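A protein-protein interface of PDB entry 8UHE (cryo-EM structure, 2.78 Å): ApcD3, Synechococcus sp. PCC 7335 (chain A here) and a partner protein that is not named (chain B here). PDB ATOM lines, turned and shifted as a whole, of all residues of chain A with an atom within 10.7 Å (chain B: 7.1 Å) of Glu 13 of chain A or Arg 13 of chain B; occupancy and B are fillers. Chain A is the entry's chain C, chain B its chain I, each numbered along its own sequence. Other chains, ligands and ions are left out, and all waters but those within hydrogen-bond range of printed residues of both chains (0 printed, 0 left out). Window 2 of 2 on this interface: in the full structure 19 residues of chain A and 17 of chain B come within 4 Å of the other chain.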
ATOM      1  N   VAL A   4     -22.629 -25.042  13.734  1.00  0.00           N
ATOM      2  CA  VAL A   4     -21.580 -24.993  12.722  1.00  0.00           C
ATOM      3  C   VAL A   4     -21.721 -26.158  11.753  1.00  0.00           C
ATOM      4  O   VAL A   4     -21.475 -26.014  10.554  1.00  0.00           O
ATOM      5  CB  VAL A   4     -20.195 -24.979  13.391  1.00  0.00           C
ATOM      6  CG1 VAL A   4     -19.149 -24.514  12.404  1.00  0.00           C
ATOM      7  CG2 VAL A   4     -20.215 -24.090  14.623  1.00  0.00           C
ATOM      8  N   LYS A   5     -22.126 -27.324  12.262  1.00  0.00           N
ATOM      9  CA  LYS A   5     -22.359 -28.490  11.414  1.00  0.00           C
ATOM     10  C   LYS A   5     -23.464 -28.232  10.394  1.00  0.00           C
ATOM     11  O   LYS A   5     -23.292 -28.496   9.196  1.00  0.00           O
ATOM     12  CB  LYS A   5     -22.710 -29.689  12.294  1.00  0.00           C
ATOM     13  CG  LYS A   5     -23.466 -30.794  11.594  1.00  0.00           C
ATOM     14  CD  LYS A   5     -22.571 -31.536  10.640  1.00  0.00           C
ATOM     15  CE  LYS A   5     -22.448 -32.970  11.058  1.00  0.00           C
ATOM     16  NZ  LYS A   5     -21.325 -33.571  10.336  1.00  0.00           N
ATOM     17  N   GLN A   6     -24.607 -27.714  10.856  1.00  0.00           N
ATOM     18  CA  GLN A   6     -25.721 -27.432   9.956  1.00  0.00           C
ATOM     19  C   GLN A   6     -25.353 -26.350   8.951  1.00  0.00           C
ATOM     20  O   GLN A   6     -25.719 -26.435   7.772  1.00  0.00           O
ATOM     21  CB  GLN A   6     -26.954 -27.027  10.765  1.00  0.00           C
ATOM     22  CG  GLN A   6     -28.155 -26.620   9.927  1.00  0.00           C
ATOM     23  CD  GLN A   6     -28.754 -27.780   9.160  1.00  0.00           C
ATOM     24  OE1 GLN A   6     -29.403 -28.652   9.736  1.00  0.00           O
ATOM     25  NE2 GLN A   6     -28.545 -27.792   7.849  1.00  0.00           N
ATOM     26  N   ILE A   7     -24.597 -25.341   9.394  1.00  0.00           N
ATOM     27  CA  ILE A   7     -24.181 -24.268   8.493  1.00  0.00           C
ATOM     28  C   ILE A   7     -23.211 -24.787   7.436  1.00  0.00           C
ATOM     29  O   ILE A   7     -23.332 -24.450   6.254  1.00  0.00           O
ATOM     30  CB  ILE A   7     -23.593 -23.103   9.308  1.00  0.00           C
ATOM     31  CG1 ILE A   7     -24.735 -22.243   9.835  1.00  0.00           C
ATOM     32  CG2 ILE A   7     -22.641 -22.258   8.479  1.00  0.00           C
ATOM     33  CD1 ILE A   7     -24.393 -21.507  11.059  1.00  0.00           C
ATOM     34  N   ILE A   8     -22.253 -25.630   7.838  1.00  0.00           N
ATOM     35  CA  ILE A   8     -21.286 -26.188   6.894  1.00  0.00           C
ATOM     36  C   ILE A   8     -21.984 -27.093   5.884  1.00  0.00           C
ATOM     37  O   ILE A   8     -21.682 -27.054   4.684  1.00  0.00           O
ATOM     38  CB  ILE A   8     -20.163 -26.924   7.655  1.00  0.00           C
ATOM     39  CG1 ILE A   8     -19.207 -25.925   8.310  1.00  0.00           C
ATOM     40  CG2 ILE A   8     -19.364 -27.836   6.737  1.00  0.00           C
ATOM     41  CD1 ILE A   8     -18.786 -24.805   7.407  1.00  0.00           C
ATOM     42  N   SER A   9     -22.945 -27.899   6.347  1.00  0.00           N
ATOM     43  CA  SER A   9     -23.699 -28.761   5.438  1.00  0.00           C
ATOM     44  C   SER A   9     -24.515 -27.941   4.440  1.00  0.00           C
ATOM     45  O   SER A   9     -24.496 -28.213   3.231  1.00  0.00           O
ATOM     46  CB  SER A   9     -24.605 -29.692   6.241  1.00  0.00           C
ATOM     47  OG  SER A   9     -25.782 -30.006   5.519  1.00  0.00           O
ATOM     48  N   ASN A  10     -25.212 -26.909   4.928  1.00  0.00           N
ATOM     49  CA  ASN A  10     -26.009 -26.064   4.044  1.00  0.00           C
ATOM     50  C   ASN A  10     -25.144 -25.258   3.081  1.00  0.00           C
ATOM     51  O   ASN A  10     -25.571 -24.982   1.954  1.00  0.00           O
ATOM     52  CB  ASN A  10     -26.887 -25.129   4.872  1.00  0.00           C
ATOM     53  CG  ASN A  10     -28.305 -25.632   4.996  1.00  0.00           C
ATOM     54  OD1 ASN A  10     -28.869 -25.676   6.088  1.00  0.00           O
ATOM     55  ND2 ASN A  10     -28.893 -26.018   3.869  1.00  0.00           N
ATOM     56  N   ALA A  11     -23.941 -24.866   3.502  1.00  0.00           N
ATOM     57  CA  ALA A  11     -23.070 -24.085   2.632  1.00  0.00           C
ATOM     58  C   ALA A  11     -22.420 -24.961   1.572  1.00  0.00           C
ATOM     59  O   ALA A  11     -22.264 -24.541   0.419  1.00  0.00           O
ATOM     60  CB  ALA A  11     -22.007 -23.368   3.460  1.00  0.00           C
ATOM     61  N   ASP A  12     -22.027 -26.180   1.944  1.00  0.00           N
ATOM     62  CA  ASP A  12     -21.443 -27.097   0.979  1.00  0.00           C
ATOM     63  C   ASP A  12     -22.481 -27.678   0.034  1.00  0.00           C
ATOM     64  O   ASP A  12     -22.112 -28.179  -1.034  1.00  0.00           O
ATOM     65  CB  ASP A  12     -20.719 -28.223   1.707  1.00  0.00           C
ATOM     66  CG  ASP A  12     -19.669 -28.882   0.852  1.00  0.00           C
ATOM     67  OD1 ASP A  12     -19.353 -28.360  -0.238  1.00  0.00           O
ATOM     68  OD2 ASP A  12     -19.174 -29.945   1.269  1.00  0.00           O
ATOM     69  N   GLU A  13     -23.763 -27.644   0.409  1.00  0.00           N
ATOM     70  CA  GLU A  13     -24.810 -28.065  -0.516  1.00  0.00           C
ATOM     71  C   GLU A  13     -24.843 -27.174  -1.753  1.00  0.00           C
ATOM     72  O   GLU A  13     -24.872 -27.665  -2.888  1.00  0.00           O
ATOM     73  CB  GLU A  13     -26.164 -28.049   0.185  1.00  0.00           C
ATOM     74  CG  GLU A  13     -27.075 -29.177  -0.228  1.00  0.00           C
ATOM     75  CD  GLU A  13     -27.936 -29.660   0.914  1.00  0.00           C
ATOM     76  OE1 GLU A  13     -27.511 -30.595   1.624  1.00  0.00           O
ATOM     77  OE2 GLU A  13     -29.036 -29.101   1.105  1.00  0.00           O
ATOM     78  N   GLU A  14     -24.808 -25.861  -1.551  1.00  0.00           N
ATOM     79  CA  GLU A  14     -24.844 -24.901  -2.642  1.00  0.00           C
ATOM     80  C   GLU A  14     -23.456 -24.559  -3.163  1.00  0.00           C
ATOM     81  O   GLU A  14     -23.330 -23.645  -3.988  1.00  0.00           O
ATOM     82  CB  GLU A  14     -25.567 -23.629  -2.197  1.00  0.00           C
ATOM     83  CG  GLU A  14     -26.985 -23.869  -1.714  1.00  0.00           C
ATOM     84  CD  GLU A  14     -27.951 -24.111  -2.856  1.00  0.00           C
ATOM     85  OE1 GLU A  14     -27.988 -23.283  -3.791  1.00  0.00           O
ATOM     86  OE2 GLU A  14     -28.670 -25.132  -2.823  1.00  0.00           O
ATOM     87  N   LEU A  15     -22.425 -25.274  -2.690  1.00  0.00           N
ATOM     88  CA  LEU A  15     -21.038 -25.114  -3.139  1.00  0.00           C
ATOM     89  C   LEU A  15     -20.548 -23.683  -2.936  1.00  0.00           C
ATOM     90  O   LEU A  15     -19.865 -23.112  -3.789  1.00  0.00           O
ATOM     91  CB  LEU A  15     -20.872 -25.544  -4.599  1.00  0.00           C
ATOM     92  CG  LEU A  15     -21.332 -26.940  -5.024  1.00  0.00           C
ATOM     93  CD1 LEU A  15     -22.710 -26.912  -5.670  1.00  0.00           C
ATOM     94  CD2 LEU A  15     -20.326 -27.518  -5.988  1.00  0.00           C
ATOM     95  N   ARG A  16     -20.913 -23.095  -1.802  1.00  0.00           N
ATOM     96  CA  ARG A  16     -20.634 -21.696  -1.525  1.00  0.00           C
ATOM     97  C   ARG A  16     -20.066 -21.542  -0.123  1.00  0.00           C
ATOM     98  O   ARG A  16     -20.321 -22.357   0.766  1.00  0.00           O
ATOM     99  CB  ARG A  16     -21.897 -20.837  -1.663  1.00  0.00           C
ATOM    100  CG  ARG A  16     -23.075 -21.356  -0.865  1.00  0.00           C
ATOM    101  CD  ARG A  16     -23.455 -20.436   0.279  1.00  0.00           C
ATOM    102  NE  ARG A  16     -24.698 -20.859   0.910  1.00  0.00           N
ATOM    103  CZ  ARG A  16     -24.883 -20.959   2.219  1.00  0.00           C
ATOM    104  NH1 ARG A  16     -23.928 -20.645   3.079  1.00  0.00           N
ATOM    105  NH2 ARG A  16     -26.056 -21.388   2.678  1.00  0.00           N
ATOM    106  N   TYR A  17     -19.286 -20.481   0.052  1.00  0.00           N
ATOM    107  CA  TYR A  17     -18.755 -20.129   1.355  1.00  0.00           C
ATOM    108  C   TYR A  17     -19.888 -19.697   2.286  1.00  0.00           C
ATOM    109  O   TYR A  17     -20.912 -19.188   1.824  1.00  0.00           O
ATOM    110  CB  TYR A  17     -17.749 -18.997   1.213  1.00  0.00           C
ATOM    111  CG  TYR A  17     -16.410 -19.416   0.666  1.00  0.00           C
ATOM    112  CD1 TYR A  17     -15.430 -19.941   1.499  1.00  0.00           C
ATOM    113  CD2 TYR A  17     -16.124 -19.281  -0.684  1.00  0.00           C
ATOM    114  CE1 TYR A  17     -14.201 -20.319   0.997  1.00  0.00           C
ATOM    115  CE2 TYR A  17     -14.906 -19.657  -1.193  1.00  0.00           C
ATOM    116  CZ  TYR A  17     -13.949 -20.174  -0.352  1.00  0.00           C
ATOM    117  OH  TYR A  17     -12.735 -20.546  -0.872  1.00  0.00           O
ATOM    118  N   PRO A  18     -19.732 -19.893   3.598  1.00  0.00           N
ATOM    119  CA  PRO A  18     -20.766 -19.436   4.538  1.00  0.00           C
ATOM    120  C   PRO A  18     -20.941 -17.923   4.500  1.00  0.00           C
ATOM    121  O   PRO A  18     -19.969 -17.165   4.484  1.00  0.00           O
ATOM    122  CB  PRO A  18     -20.243 -19.906   5.901  1.00  0.00           C
ATOM    123  CG  PRO A  18     -19.246 -20.964   5.592  1.00  0.00           C
ATOM    124  CD  PRO A  18     -18.633 -20.591   4.289  1.00  0.00           C
ATOM    125  N   GLN A  99     -29.740 -31.911  16.751  1.00  0.00           N
ATOM    126  CA  GLN A  99     -29.099 -33.001  16.018  1.00  0.00           C
ATOM    127  C   GLN A  99     -28.747 -34.209  16.887  1.00  0.00           C
ATOM    128  O   GLN A  99     -29.052 -35.339  16.466  1.00  0.00           O
ATOM    129  CB  GLN A  99     -27.874 -32.465  15.266  1.00  0.00           C
ATOM    130  CG  GLN A  99     -28.183 -31.438  14.195  1.00  0.00           C
ATOM    131  CD  GLN A  99     -27.994 -32.001  12.804  1.00  0.00           C
ATOM    132  OE1 GLN A  99     -28.425 -33.116  12.515  1.00  0.00           O
ATOM    133  NE2 GLN A  99     -27.334 -31.241  11.939  1.00  0.00           N
ATOM    134  N   ARG A 102     -32.127 -36.307  17.663  1.00  0.00           N
ATOM    135  CA  ARG A 102     -32.668 -36.960  16.477  1.00  0.00           C
ATOM    136  C   ARG A 102     -31.747 -38.066  15.984  1.00  0.00           C
ATOM    137  O   ARG A 102     -32.109 -39.249  16.015  1.00  0.00           O
ATOM    138  CB  ARG A 102     -32.910 -35.933  15.376  1.00  0.00           C
ATOM    139  CG  ARG A 102     -34.202 -35.152  15.521  1.00  0.00           C
ATOM    140  CD  ARG A 102     -34.376 -34.105  14.421  1.00  0.00           C
ATOM    141  NE  ARG A 102     -33.283 -33.141  14.351  1.00  0.00           N
ATOM    142  CZ  ARG A 102     -32.273 -33.193  13.492  1.00  0.00           C
ATOM    143  NH1 ARG A 102     -32.156 -34.182  12.623  1.00  0.00           N
ATOM    144  NH2 ARG A 102     -31.359 -32.229  13.509  1.00  0.00           N
ATOM    145  N   VAL B   7     -33.573 -21.085   8.660  1.00  0.00           N
ATOM    146  CA  VAL B   7     -33.814 -22.052   9.722  1.00  0.00           C
ATOM    147  C   VAL B   7     -35.235 -22.608   9.614  1.00  0.00           C
ATOM    148  O   VAL B   7     -35.478 -23.794   9.888  1.00  0.00           O
ATOM    149  CB  VAL B   7     -33.487 -21.425  11.093  1.00  0.00           C
ATOM    150  CG1 VAL B   7     -34.619 -20.566  11.666  1.00  0.00           C
ATOM    151  CG2 VAL B   7     -33.029 -22.483  12.042  1.00  0.00           C
ATOM    152  N   ILE B   8     -36.173 -21.788   9.120  1.00  0.00           N
ATOM    153  CA  ILE B   8     -37.507 -22.266   8.775  1.00  0.00           C
ATOM    154  C   ILE B   8     -37.431 -23.287   7.647  1.00  0.00           C
ATOM    155  O   ILE B   8     -38.068 -24.344   7.704  1.00  0.00           O
ATOM    156  CB  ILE B   8     -38.409 -21.070   8.411  1.00  0.00           C
ATOM    157  CG1 ILE B   8     -38.946 -20.404   9.676  1.00  0.00           C
ATOM    158  CG2 ILE B   8     -39.550 -21.479   7.484  1.00  0.00           C
ATOM    159  CD1 ILE B   8     -39.596 -19.069   9.423  1.00  0.00           C
ATOM    160  N   ALA B   9     -36.633 -22.994   6.615  1.00  0.00           N
ATOM    161  CA  ALA B   9     -36.496 -23.908   5.483  1.00  0.00           C
ATOM    162  C   ALA B   9     -35.840 -25.222   5.899  1.00  0.00           C
ATOM    163  O   ALA B   9     -36.214 -26.293   5.406  1.00  0.00           O
ATOM    164  CB  ALA B   9     -35.697 -23.239   4.366  1.00  0.00           C
ATOM    165  N   THR B  10     -34.859 -25.157   6.802  1.00  0.00           N
ATOM    166  CA  THR B  10     -34.194 -26.358   7.295  1.00  0.00           C
ATOM    167  C   THR B  10     -35.139 -27.218   8.127  1.00  0.00           C
ATOM    168  O   THR B  10     -35.138 -28.450   7.999  1.00  0.00           O
ATOM    169  CB  THR B  10     -32.961 -25.969   8.113  1.00  0.00           C
ATOM    170  OG1 THR B  10     -32.061 -25.219   7.289  1.00  0.00           O
ATOM    171  CG2 THR B  10     -32.243 -27.203   8.645  1.00  0.00           C
ATOM    172  N   ALA B  11     -35.952 -26.591   8.985  1.00  0.00           N
ATOM    173  CA  ALA B  11     -36.962 -27.351   9.716  1.00  0.00           C
ATOM    174  C   ALA B  11     -38.011 -27.923   8.770  1.00  0.00           C
ATOM    175  O   ALA B  11     -38.550 -29.010   9.011  1.00  0.00           O
ATOM    176  CB  ALA B  11     -37.618 -26.474  10.779  1.00  0.00           C
ATOM    177  N   ASP B  12     -38.315 -27.202   7.689  1.00  0.00           N
ATOM    178  CA  ASP B  12     -39.270 -27.703   6.708  1.00  0.00           C
ATOM    179  C   ASP B  12     -38.727 -28.920   5.974  1.00  0.00           C
ATOM    180  O   ASP B  12     -39.472 -29.861   5.687  1.00  0.00           O
ATOM    181  CB  ASP B  12     -39.626 -26.598   5.716  1.00  0.00           C
ATOM    182  CG  ASP B  12     -40.953 -26.837   5.037  1.00  0.00           C
ATOM    183  OD1 ASP B  12     -41.666 -27.785   5.428  1.00  0.00           O
ATOM    184  OD2 ASP B  12     -41.292 -26.074   4.114  1.00  0.00           O
ATOM    185  N   ARG B  13     -37.431 -28.918   5.663  1.00  0.00           N
ATOM    186  CA  ARG B  13     -36.841 -30.004   4.886  1.00  0.00           C
ATOM    187  C   ARG B  13     -36.809 -31.303   5.679  1.00  0.00           C
ATOM    188  O   ARG B  13     -37.298 -32.339   5.216  1.00  0.00           O
ATOM    189  CB  ARG B  13     -35.436 -29.618   4.454  1.00  0.00           C
ATOM    190  CG  ARG B  13     -35.395 -28.637   3.322  1.00  0.00           C
ATOM    191  CD  ARG B  13     -33.966 -28.472   2.898  1.00  0.00           C
ATOM    192  NE  ARG B  13     -33.377 -29.775   2.632  1.00  0.00           N
ATOM    193  CZ  ARG B  13     -32.238 -29.967   1.985  1.00  0.00           C
ATOM    194  NH1 ARG B  13     -31.539 -28.953   1.502  1.00  0.00           N
ATOM    195  NH2 ARG B  13     -31.788 -31.207   1.817  1.00  0.00           N
ATOM    196  N   GLU B  14     -36.218 -31.271   6.871  1.00  0.00           N
ATOM    197  CA  GLU B  14     -36.252 -32.406   7.789  1.00  0.00           C
ATOM    198  C   GLU B  14     -37.423 -32.157   8.730  1.00  0.00           C
ATOM    199  O   GLU B  14     -37.272 -31.576   9.800  1.00  0.00           O
ATOM    200  CB  GLU B  14     -34.933 -32.529   8.541  1.00  0.00           C
ATOM    201  CG  GLU B  14     -33.735 -32.811   7.650  1.00  0.00           C
ATOM    202  CD  GLU B  14     -32.467 -33.107   8.432  1.00  0.00           C
ATOM    203  OE1 GLU B  14     -32.442 -32.862   9.657  1.00  0.00           O
ATOM    204  OE2 GLU B  14     -31.495 -33.588   7.815  1.00  0.00           O
ATOM    205  N   VAL B  15     -38.608 -32.616   8.306  1.00  0.00           N
ATOM    206  CA  VAL B  15     -39.906 -32.157   8.812  1.00  0.00           C
ATOM    207  C   VAL B  15     -40.065 -32.246  10.322  1.00  0.00           C
ATOM    208  O   VAL B  15     -40.063 -33.335  10.911  1.00  0.00           O
ATOM    209  CB  VAL B  15     -41.055 -32.912   8.125  1.00  0.00           C
ATOM    210  CG1 VAL B  15     -41.320 -32.315   6.803  1.00  0.00           C
ATOM    211  CG2 VAL B  15     -40.664 -34.329   7.915  1.00  0.00           C
ATOM    212  N   ARG B  16     -40.229 -31.079  10.938  1.00  0.00           N
ATOM    213  CA  ARG B  16     -40.319 -30.889  12.375  1.00  0.00           C
ATOM    214  C   ARG B  16     -40.643 -29.426  12.617  1.00  0.00           C
ATOM    215  O   ARG B  16     -40.814 -28.657  11.666  1.00  0.00           O
ATOM    216  CB  ARG B  16     -39.012 -31.257  13.075  1.00  0.00           C
ATOM    217  CG  ARG B  16     -37.880 -30.397  12.616  1.00  0.00           C
ATOM    218  CD  ARG B  16     -36.531 -30.896  13.081  1.00  0.00           C
ATOM    219  NE  ARG B  16     -35.454 -30.287  12.310  1.00  0.00           N
ATOM    220  CZ  ARG B  16     -35.061 -29.025  12.419  1.00  0.00           C
ATOM    221  NH1 ARG B  16     -35.625 -28.194  13.281  1.00  0.00           N
ATOM    222  NH2 ARG B  16     -34.076 -28.583  11.643  1.00  0.00           N
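The side-chain amide nitrogen of Gln 6 of chain A is in hydrogen-bond range of the side-chain amide oxygen of Asn 10 of chain A, at 2.8 Å. The side-chain amide oxygen of Gln 99 of chain A sits at hydrogen-bond distance from the guanidinium group of Arg 102 of chain A, 3.2 Å away. The backbone carbonyl oxygen of Glu 14 of chain B lies close to the guanidinium group of Arg 16 of chain B (3.4 Å).
Thr 10 of chain B touches Gln 6 of chain A (CG2 to OE1, 3.4 Å).
Glu 13 of chain A touches one residue of chain B. Arg 13 of chain B touches just one residue of chain A: Glu 13 (2.5 Å). Of chain A, only Gln 6 (3.4 Å) and Asn 10 (3.4 Å) come within 4 Å of Thr 10 of chain B. No residue of chain A comes within 4 Å of Ala 11 of chain B. No residue of chain A comes within 4 Å of Val 15 of chain B. Printed residues of chain B within 4 Å of Asn 10 of chain A: Thr 10. Printed residues of chain B within 4 Å of Arg 102 of chain A: Glu 14 (3.3 Å). Of the printed residues of chain B, Gln 6 of chain A touches Thr 10. Arg 16 of chain A touches none of the printed residues of chain B. The nearest printed residue of chain B that does not touch Glu 13 of chain A is Thr 10 of chain B (7.9 Å).
OD1 of Asn 10 of chain A is in hydrogen-bond range of OG1 of Thr 10 of chain B. The guanidinium group of Arg 13 of chain B lies within salt-bridge range of the side-chain carboxylate of Glu 13 of chain A, at 2.5 Å. The guanidinium group (NH1) of Arg 102 of chain A lies within salt-bridge range of the side-chain carboxylate (OE1) of Glu 14 of chain B, at 3.3 Å.
Along chain A the printed residues that touch a printed residue of chain B span positions 6 to 102. Among the printed residues, 4 pairs touch across the chains. Among the printed residues, Asp or Glu carboxylates within 4 Å of a Lys or Arg side-chain nitrogen of the other chain: Glu 13 of chain A with Arg 13 of chain B (2.5 Å) and Arg 102 of chain A with Glu 14 of chain B (3.3 Å).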
